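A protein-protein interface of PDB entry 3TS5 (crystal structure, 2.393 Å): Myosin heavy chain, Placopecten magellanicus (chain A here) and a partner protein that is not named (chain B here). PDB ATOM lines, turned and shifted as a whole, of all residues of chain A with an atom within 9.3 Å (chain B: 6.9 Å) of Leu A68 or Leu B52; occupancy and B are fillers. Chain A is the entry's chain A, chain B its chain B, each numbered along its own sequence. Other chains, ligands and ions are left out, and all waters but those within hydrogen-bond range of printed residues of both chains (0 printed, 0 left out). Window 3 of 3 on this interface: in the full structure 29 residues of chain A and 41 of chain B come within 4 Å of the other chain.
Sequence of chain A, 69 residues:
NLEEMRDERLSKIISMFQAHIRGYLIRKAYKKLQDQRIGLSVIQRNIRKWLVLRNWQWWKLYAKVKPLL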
ATOM      1  N   GLN A  57      -3.901  -4.093  16.317  1.00  0.00           N
ATOM      2  CA  GLN A  57      -2.750  -3.551  17.018  1.00  0.00           C
ATOM      3  C   GLN A  57      -3.051  -3.147  18.468  1.00  0.00           C
ATOM      4  O   GLN A  57      -2.222  -3.348  19.357  1.00  0.00           O
ATOM      5  CB  GLN A  57      -2.158  -2.376  16.222  1.00  0.00           C
ATOM      6  CG  GLN A  57      -0.801  -1.899  16.742  1.00  0.00           C
ATOM      7  CD  GLN A  57       0.252  -2.994  16.754  1.00  0.00           C
ATOM      8  OE1 GLN A  57       0.646  -3.479  17.824  1.00  0.00           O
ATOM      9  NE2 GLN A  57       0.710  -3.393  15.568  1.00  0.00           N
ATOM     10  N   LYS A  60      -2.866  -6.355  20.502  1.00  0.00           N
ATOM     11  CA  LYS A  60      -1.504  -6.867  20.669  1.00  0.00           C
ATOM     12  C   LYS A  60      -0.788  -6.122  21.792  1.00  0.00           C
ATOM     13  O   LYS A  60      -0.095  -6.730  22.617  1.00  0.00           O
ATOM     14  CB  LYS A  60      -0.718  -6.755  19.359  1.00  0.00           C
ATOM     15  CG  LYS A  60      -1.248  -7.654  18.244  1.00  0.00           C
ATOM     16  CD  LYS A  60      -0.656  -7.276  16.900  1.00  0.00           C
ATOM     17  CE  LYS A  60      -0.670  -8.461  15.945  1.00  0.00           C
ATOM     18  NZ  LYS A  60      -0.222  -8.072  14.573  1.00  0.00           N
ATOM     19  N   LEU A  61      -0.958  -4.802  21.801  1.00  0.00           N
ATOM     20  CA  LEU A  61      -0.522  -3.967  22.900  1.00  0.00           C
ATOM     21  C   LEU A  61      -1.174  -4.456  24.197  1.00  0.00           C
ATOM     22  O   LEU A  61      -0.497  -4.848  25.158  1.00  0.00           O
ATOM     23  CB  LEU A  61      -0.922  -2.507  22.647  1.00  0.00           C
ATOM     24  CG  LEU A  61      -0.440  -1.539  23.736  1.00  0.00           C
ATOM     25  CD1 LEU A  61       1.048  -1.717  23.917  1.00  0.00           C
ATOM     26  CD2 LEU A  61      -0.784  -0.069  23.445  1.00  0.00           C
ATOM     27  N   TYR A  62      -2.500  -4.420  24.210  1.00  0.00           N
ATOM     28  CA  TYR A  62      -3.252  -4.809  25.380  1.00  0.00           C
ATOM     29  C   TYR A  62      -2.750  -6.133  25.986  1.00  0.00           C
ATOM     30  O   TYR A  62      -2.585  -6.250  27.200  1.00  0.00           O
ATOM     31  CB  TYR A  62      -4.731  -4.904  25.028  1.00  0.00           C
ATOM     32  CG  TYR A  62      -5.622  -5.065  26.224  1.00  0.00           C
ATOM     33  CD1 TYR A  62      -6.218  -3.959  26.830  1.00  0.00           C
ATOM     34  CD2 TYR A  62      -5.885  -6.334  26.753  1.00  0.00           C
ATOM     35  CE1 TYR A  62      -7.058  -4.103  27.945  1.00  0.00           C
ATOM     36  CE2 TYR A  62      -6.726  -6.497  27.870  1.00  0.00           C
ATOM     37  CZ  TYR A  62      -7.307  -5.376  28.457  1.00  0.00           C
ATOM     38  OH  TYR A  62      -8.132  -5.526  29.545  1.00  0.00           O
ATOM     39  N   ALA A  63      -2.502  -7.129  25.142  1.00  0.00           N
ATOM     40  CA  ALA A  63      -2.130  -8.437  25.654  1.00  0.00           C
ATOM     41  C   ALA A  63      -0.693  -8.495  26.191  1.00  0.00           C
ATOM     42  O   ALA A  63      -0.356  -9.372  26.988  1.00  0.00           O
ATOM     43  CB  ALA A  63      -2.320  -9.489  24.571  1.00  0.00           C
ATOM     44  N   LYS A  64       0.151  -7.570  25.751  1.00  0.00           N
ATOM     45  CA  LYS A  64       1.499  -7.446  26.301  1.00  0.00           C
ATOM     46  C   LYS A  64       1.498  -6.708  27.653  1.00  0.00           C
ATOM     47  O   LYS A  64       2.391  -6.898  28.483  1.00  0.00           O
ATOM     48  CB  LYS A  64       2.409  -6.731  25.300  1.00  0.00           C
ATOM     49  CG  LYS A  64       2.963  -7.642  24.220  1.00  0.00           C
ATOM     50  CD  LYS A  64       3.612  -6.820  23.114  1.00  0.00           C
ATOM     51  CE  LYS A  64       4.453  -7.685  22.175  1.00  0.00           C
ATOM     52  NZ  LYS A  64       5.540  -6.879  21.517  1.00  0.00           N
ATOM     53  N   VAL A  65       0.490  -5.864  27.851  1.00  0.00           N
ATOM     54  CA  VAL A  65       0.326  -5.091  29.071  1.00  0.00           C
ATOM     55  C   VAL A  65      -0.376  -5.907  30.170  1.00  0.00           C
ATOM     56  O   VAL A  65      -0.142  -5.700  31.359  1.00  0.00           O
ATOM     57  CB  VAL A  65      -0.479  -3.801  28.775  1.00  0.00           C
ATOM     58  CG1 VAL A  65      -0.790  -3.024  30.042  1.00  0.00           C
ATOM     59  CG2 VAL A  65       0.272  -2.930  27.784  1.00  0.00           C
ATOM     60  N   LYS A  66      -1.226  -6.845  29.769  1.00  0.00           N
ATOM     61  CA  LYS A  66      -2.029  -7.583  30.732  1.00  0.00           C
ATOM     62  C   LYS A  66      -1.193  -8.333  31.793  1.00  0.00           C
ATOM     63  O   LYS A  66      -1.541  -8.329  32.975  1.00  0.00           O
ATOM     64  CB  LYS A  66      -3.016  -8.518  30.015  1.00  0.00           C
ATOM     65  CG  LYS A  66      -4.195  -8.950  30.877  1.00  0.00           C
ATOM     66  CD  LYS A  66      -5.071  -9.992  30.165  1.00  0.00           C
ATOM     67  CE  LYS A  66      -6.070 -10.652  31.132  1.00  0.00           C
ATOM     68  NZ  LYS A  66      -5.399 -11.127  32.395  1.00  0.00           N
ATOM     69  N   PRO A  67      -0.086  -8.971  31.378  1.00  0.00           N
ATOM     70  CA  PRO A  67       0.787  -9.693  32.319  1.00  0.00           C
ATOM     71  C   PRO A  67       1.484  -8.784  33.332  1.00  0.00           C
ATOM     72  O   PRO A  67       1.798  -9.225  34.447  1.00  0.00           O
ATOM     73  CB  PRO A  67       1.847 -10.317  31.400  1.00  0.00           C
ATOM     74  CG  PRO A  67       1.205 -10.376  30.040  1.00  0.00           C
ATOM     75  CD  PRO A  67       0.335  -9.160  29.978  1.00  0.00           C
ATOM     76  N   LEU A  68       1.751  -7.540  32.940  1.00  0.00           N
ATOM     77  CA  LEU A  68       2.439  -6.595  33.816  1.00  0.00           C
ATOM     78  C   LEU A  68       1.537  -6.033  34.906  1.00  0.00           C
ATOM     79  O   LEU A  68       2.016  -5.393  35.842  1.00  0.00           O
ATOM     80  CB  LEU A  68       2.994  -5.434  33.006  1.00  0.00           C
ATOM     81  CG  LEU A  68       3.858  -5.813  31.814  1.00  0.00           C
ATOM     82  CD1 LEU A  68       4.212  -4.559  31.044  1.00  0.00           C
ATOM     83  CD2 LEU A  68       5.105  -6.547  32.280  1.00  0.00           C
ATOM     84  N   LEU A  69       0.230  -6.241  34.764  1.00  0.00           N
ATOM     85  CA  LEU A  69      -0.722  -5.736  35.746  1.00  0.00           C
ATOM     86  C   LEU A  69      -0.602  -6.554  37.034  1.00  0.00           C
ATOM     87  O   LEU A  69      -1.237  -6.240  38.035  1.00  0.00           O
ATOM     88  CB  LEU A  69      -2.159  -5.783  35.208  1.00  0.00           C
ATOM     89  CG  LEU A  69      -2.551  -5.203  33.838  1.00  0.00           C
ATOM     90  CD1 LEU A  69      -4.056  -5.431  33.566  1.00  0.00           C
ATOM     91  CD2 LEU A  69      -2.184  -3.728  33.675  1.00  0.00           C
ATOM     92  N   GLU B  27      -7.053  -0.661  34.554  1.00  0.00           N
ATOM     93  CA  GLU B  27      -5.658  -0.893  34.901  1.00  0.00           C
ATOM     94  C   GLU B  27      -4.764  -0.706  33.688  1.00  0.00           C
ATOM     95  O   GLU B  27      -3.726  -0.043  33.763  1.00  0.00           O
ATOM     96  CB  GLU B  27      -5.456  -2.295  35.485  1.00  0.00           C
ATOM     97  CG  GLU B  27      -5.781  -2.425  36.976  1.00  0.00           C
ATOM     98  CD  GLU B  27      -5.056  -3.601  37.647  1.00  0.00           C
ATOM     99  OE1 GLU B  27      -3.908  -3.408  38.122  1.00  0.00           O
ATOM    100  OE2 GLU B  27      -5.631  -4.717  37.703  1.00  0.00           O
ATOM    101  N   MET B  31      -1.882   2.227  33.026  1.00  0.00           N
ATOM    102  CA  MET B  31      -0.468   1.991  32.771  1.00  0.00           C
ATOM    103  C   MET B  31       0.012   2.643  31.473  1.00  0.00           C
ATOM    104  O   MET B  31       1.147   3.114  31.380  1.00  0.00           O
ATOM    105  CB  MET B  31      -0.178   0.495  32.733  1.00  0.00           C
ATOM    106  CG  MET B  31       1.319   0.187  32.716  1.00  0.00           C
ATOM    107  SD  MET B  31       1.652  -1.584  32.822  1.00  0.00           S
ATOM    108  CE  MET B  31       0.820  -1.998  34.357  1.00  0.00           C
ATOM    109  N   LYS B  46       4.144   5.721  22.392  1.00  0.00           N
ATOM    110  CA  LYS B  46       5.559   5.468  22.067  1.00  0.00           C
ATOM    111  C   LYS B  46       6.282   4.957  23.300  1.00  0.00           C
ATOM    112  O   LYS B  46       7.023   3.973  23.246  1.00  0.00           O
ATOM    113  CB  LYS B  46       6.280   6.730  21.596  1.00  0.00           C
ATOM    114  CG  LYS B  46       5.841   7.310  20.262  1.00  0.00           C
ATOM    115  CD  LYS B  46       6.846   8.383  19.810  1.00  0.00           C
ATOM    116  CE  LYS B  46       6.488   9.009  18.467  1.00  0.00           C
ATOM    117  NZ  LYS B  46       7.649   9.706  17.814  1.00  0.00           N
ATOM    118  N   GLU B  47       6.055   5.651  24.412  1.00  0.00           N
ATOM    119  CA  GLU B  47       6.599   5.260  25.702  1.00  0.00           C
ATOM    120  C   GLU B  47       6.285   3.808  26.056  1.00  0.00           C
ATOM    121  O   GLU B  47       7.187   3.030  26.422  1.00  0.00           O
ATOM    122  CB  GLU B  47       6.052   6.175  26.806  1.00  0.00           C
ATOM    123  CG  GLU B  47       6.967   6.274  27.993  1.00  0.00           C
ATOM    124  CD  GLU B  47       8.410   6.526  27.561  1.00  0.00           C
ATOM    125  OE1 GLU B  47       8.630   7.391  26.670  1.00  0.00           O
ATOM    126  OE2 GLU B  47       9.311   5.833  28.095  1.00  0.00           O
ATOM    127  N   MET B  48       5.007   3.446  25.972  1.00  0.00           N
ATOM    128  CA  MET B  48       4.611   2.106  26.351  1.00  0.00           C
ATOM    129  C   MET B  48       5.234   1.069  25.424  1.00  0.00           C
ATOM    130  O   MET B  48       5.789   0.069  25.892  1.00  0.00           O
ATOM    131  CB  MET B  48       3.094   1.957  26.360  1.00  0.00           C
ATOM    132  CG  MET B  48       2.631   0.622  26.934  1.00  0.00           C
ATOM    133  SD  MET B  48       2.819   0.546  28.742  1.00  0.00           S
ATOM    134  CE  MET B  48       3.912  -0.846  28.926  1.00  0.00           C
ATOM    135  N   PHE B  49       5.151   1.303  24.114  1.00  0.00           N
ATOM    136  CA  PHE B  49       5.689   0.327  23.152  1.00  0.00           C
ATOM    137  C   PHE B  49       7.190   0.127  23.329  1.00  0.00           C
ATOM    138  O   PHE B  49       7.687  -1.005  23.306  1.00  0.00           O
ATOM    139  CB  PHE B  49       5.381   0.724  21.698  1.00  0.00           C
ATOM    140  CG  PHE B  49       4.061   0.199  21.192  1.00  0.00           C
ATOM    141  CD1 PHE B  49       3.889  -1.158  20.941  1.00  0.00           C
ATOM    142  CD2 PHE B  49       2.991   1.060  20.968  1.00  0.00           C
ATOM    143  CE1 PHE B  49       2.679  -1.643  20.475  1.00  0.00           C
ATOM    144  CE2 PHE B  49       1.789   0.585  20.512  1.00  0.00           C
ATOM    145  CZ  PHE B  49       1.627  -0.767  20.263  1.00  0.00           C
ATOM    146  N   SER B  50       7.907   1.235  23.509  1.00  0.00           N
ATOM    147  CA  SER B  50       9.355   1.166  23.680  1.00  0.00           C
ATOM    148  C   SER B  50       9.763   0.426  24.952  1.00  0.00           C
ATOM    149  O   SER B  50      10.866  -0.099  25.027  1.00  0.00           O
ATOM    150  CB  SER B  50      10.007   2.559  23.599  1.00  0.00           C
ATOM    151  OG  SER B  50       9.587   3.420  24.640  1.00  0.00           O
ATOM    152  N   SER B  51       8.870   0.372  25.939  1.00  0.00           N
ATOM    153  CA  SER B  51       9.132  -0.352  27.178  1.00  0.00           C
ATOM    154  C   SER B  51       8.933  -1.849  26.989  1.00  0.00           C
ATOM    155  O   SER B  51       9.369  -2.652  27.815  1.00  0.00           O
ATOM    156  CB  SER B  51       8.216   0.147  28.303  1.00  0.00           C
ATOM    157  OG  SER B  51       8.401   1.532  28.553  1.00  0.00           O
ATOM    158  N   LEU B  52       8.269  -2.220  25.898  1.00  0.00           N
ATOM    159  CA  LEU B  52       7.884  -3.614  25.654  1.00  0.00           C
ATOM    160  C   LEU B  52       8.732  -4.294  24.567  1.00  0.00           C
ATOM    161  O   LEU B  52       8.777  -5.518  24.468  1.00  0.00           O
ATOM    162  CB  LEU B  52       6.404  -3.675  25.260  1.00  0.00           C
ATOM    163  CG  LEU B  52       5.334  -4.015  26.295  1.00  0.00           C
ATOM    164  CD1 LEU B  52       5.901  -4.192  27.697  1.00  0.00           C
ATOM    165  CD2 LEU B  52       4.195  -2.982  26.263  1.00  0.00           C
ATOM    166  N   GLY B  53       9.390  -3.492  23.743  1.00  0.00           N
ATOM    167  CA  GLY B  53      10.199  -4.013  22.659  1.00  0.00           C
ATOM    168  C   GLY B  53      10.241  -3.036  21.501  1.00  0.00           C
ATOM    169  O   GLY B  53      10.486  -1.845  21.704  1.00  0.00           O
ATOM    170  N   ARG B  54      10.007  -3.541  20.293  1.00  0.00           N
ATOM    171  CA  ARG B  54       9.945  -2.703  19.096  1.00  0.00           C
ATOM    172  C   ARG B  54       8.889  -1.611  19.248  1.00  0.00           C
ATOM    173  O   ARG B  54       7.808  -1.839  19.800  1.00  0.00           O
ATOM    174  CB  ARG B  54       9.643  -3.563  17.857  1.00  0.00           C
ATOM    175  CG  ARG B  54       9.056  -2.809  16.660  1.00  0.00           C
ATOM    176  CD  ARG B  54       8.309  -3.770  15.721  1.00  0.00           C
ATOM    177  NE  ARG B  54       9.121  -4.947  15.400  1.00  0.00           N
ATOM    178  CZ  ARG B  54       8.674  -6.038  14.776  1.00  0.00           C
ATOM    179  NH1 ARG B  54       7.402  -6.122  14.396  1.00  0.00           N
ATOM    180  NH2 ARG B  54       9.504  -7.053  14.533  1.00  0.00           N
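Phe B49 touches Gln A57 (CZ to OE1, 3.8 Å).
Phe B49 touches Leu A61.
SD of Met B31 touches CG1 of Val A65 (3.97 Å).
O of Leu A68 touches CE of Met B31 (3.9 Å).
Leu B52 touches Leu A68.
Leu A69 touches Glu B27.
Leu A69 touches Met B31 (CD2 to CE, 3.5 Å).
Leu A68 touches just these residues of chain B: Met B31 (3.9 Å) and Leu B52 (3.8 Å).
Of the printed residues of chain A, Leu B52 touches Leu A68.
No residue of chain A comes within 4 Å of Gly B53.
Of the printed residues of chain B, Leu A61 touches Phe B49.
Printed residues of chain B within 4 Å of Val A65: Met B31 (3.97 Å).
Of the printed residues of chain A, Glu B27 touches Leu A69 (3.9 Å).
Of the printed residues of chain A, Met B31 touches Val A65, Leu A68 and Leu A69.
Of the printed residues of chain A, Phe B49 touches Gln A57 and Leu A61.
Ala A63 touches none of the printed residues of chain B.
Ser B50 touches none of the printed residues of chain A.
The nearest residue of chain B that does not touch Leu A68 is Met B48 (4.3 Å).
Of the 11 printed residues of chain B, 4 touch a printed residue of chain A.
Printed residues of chain B that touch a printed residue of chain A: Glu B27, Met B31, Phe B49 and Leu B52.
Along chain A the printed residues that touch a printed residue of chain B span positions 57 to 69.
Among the printed residues, 7 pairs touch across the chains.
Among the printed residues, no Asp or Glu carboxylate lies within 4 Å of a Lys or Arg side-chain nitrogen of the other chain.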
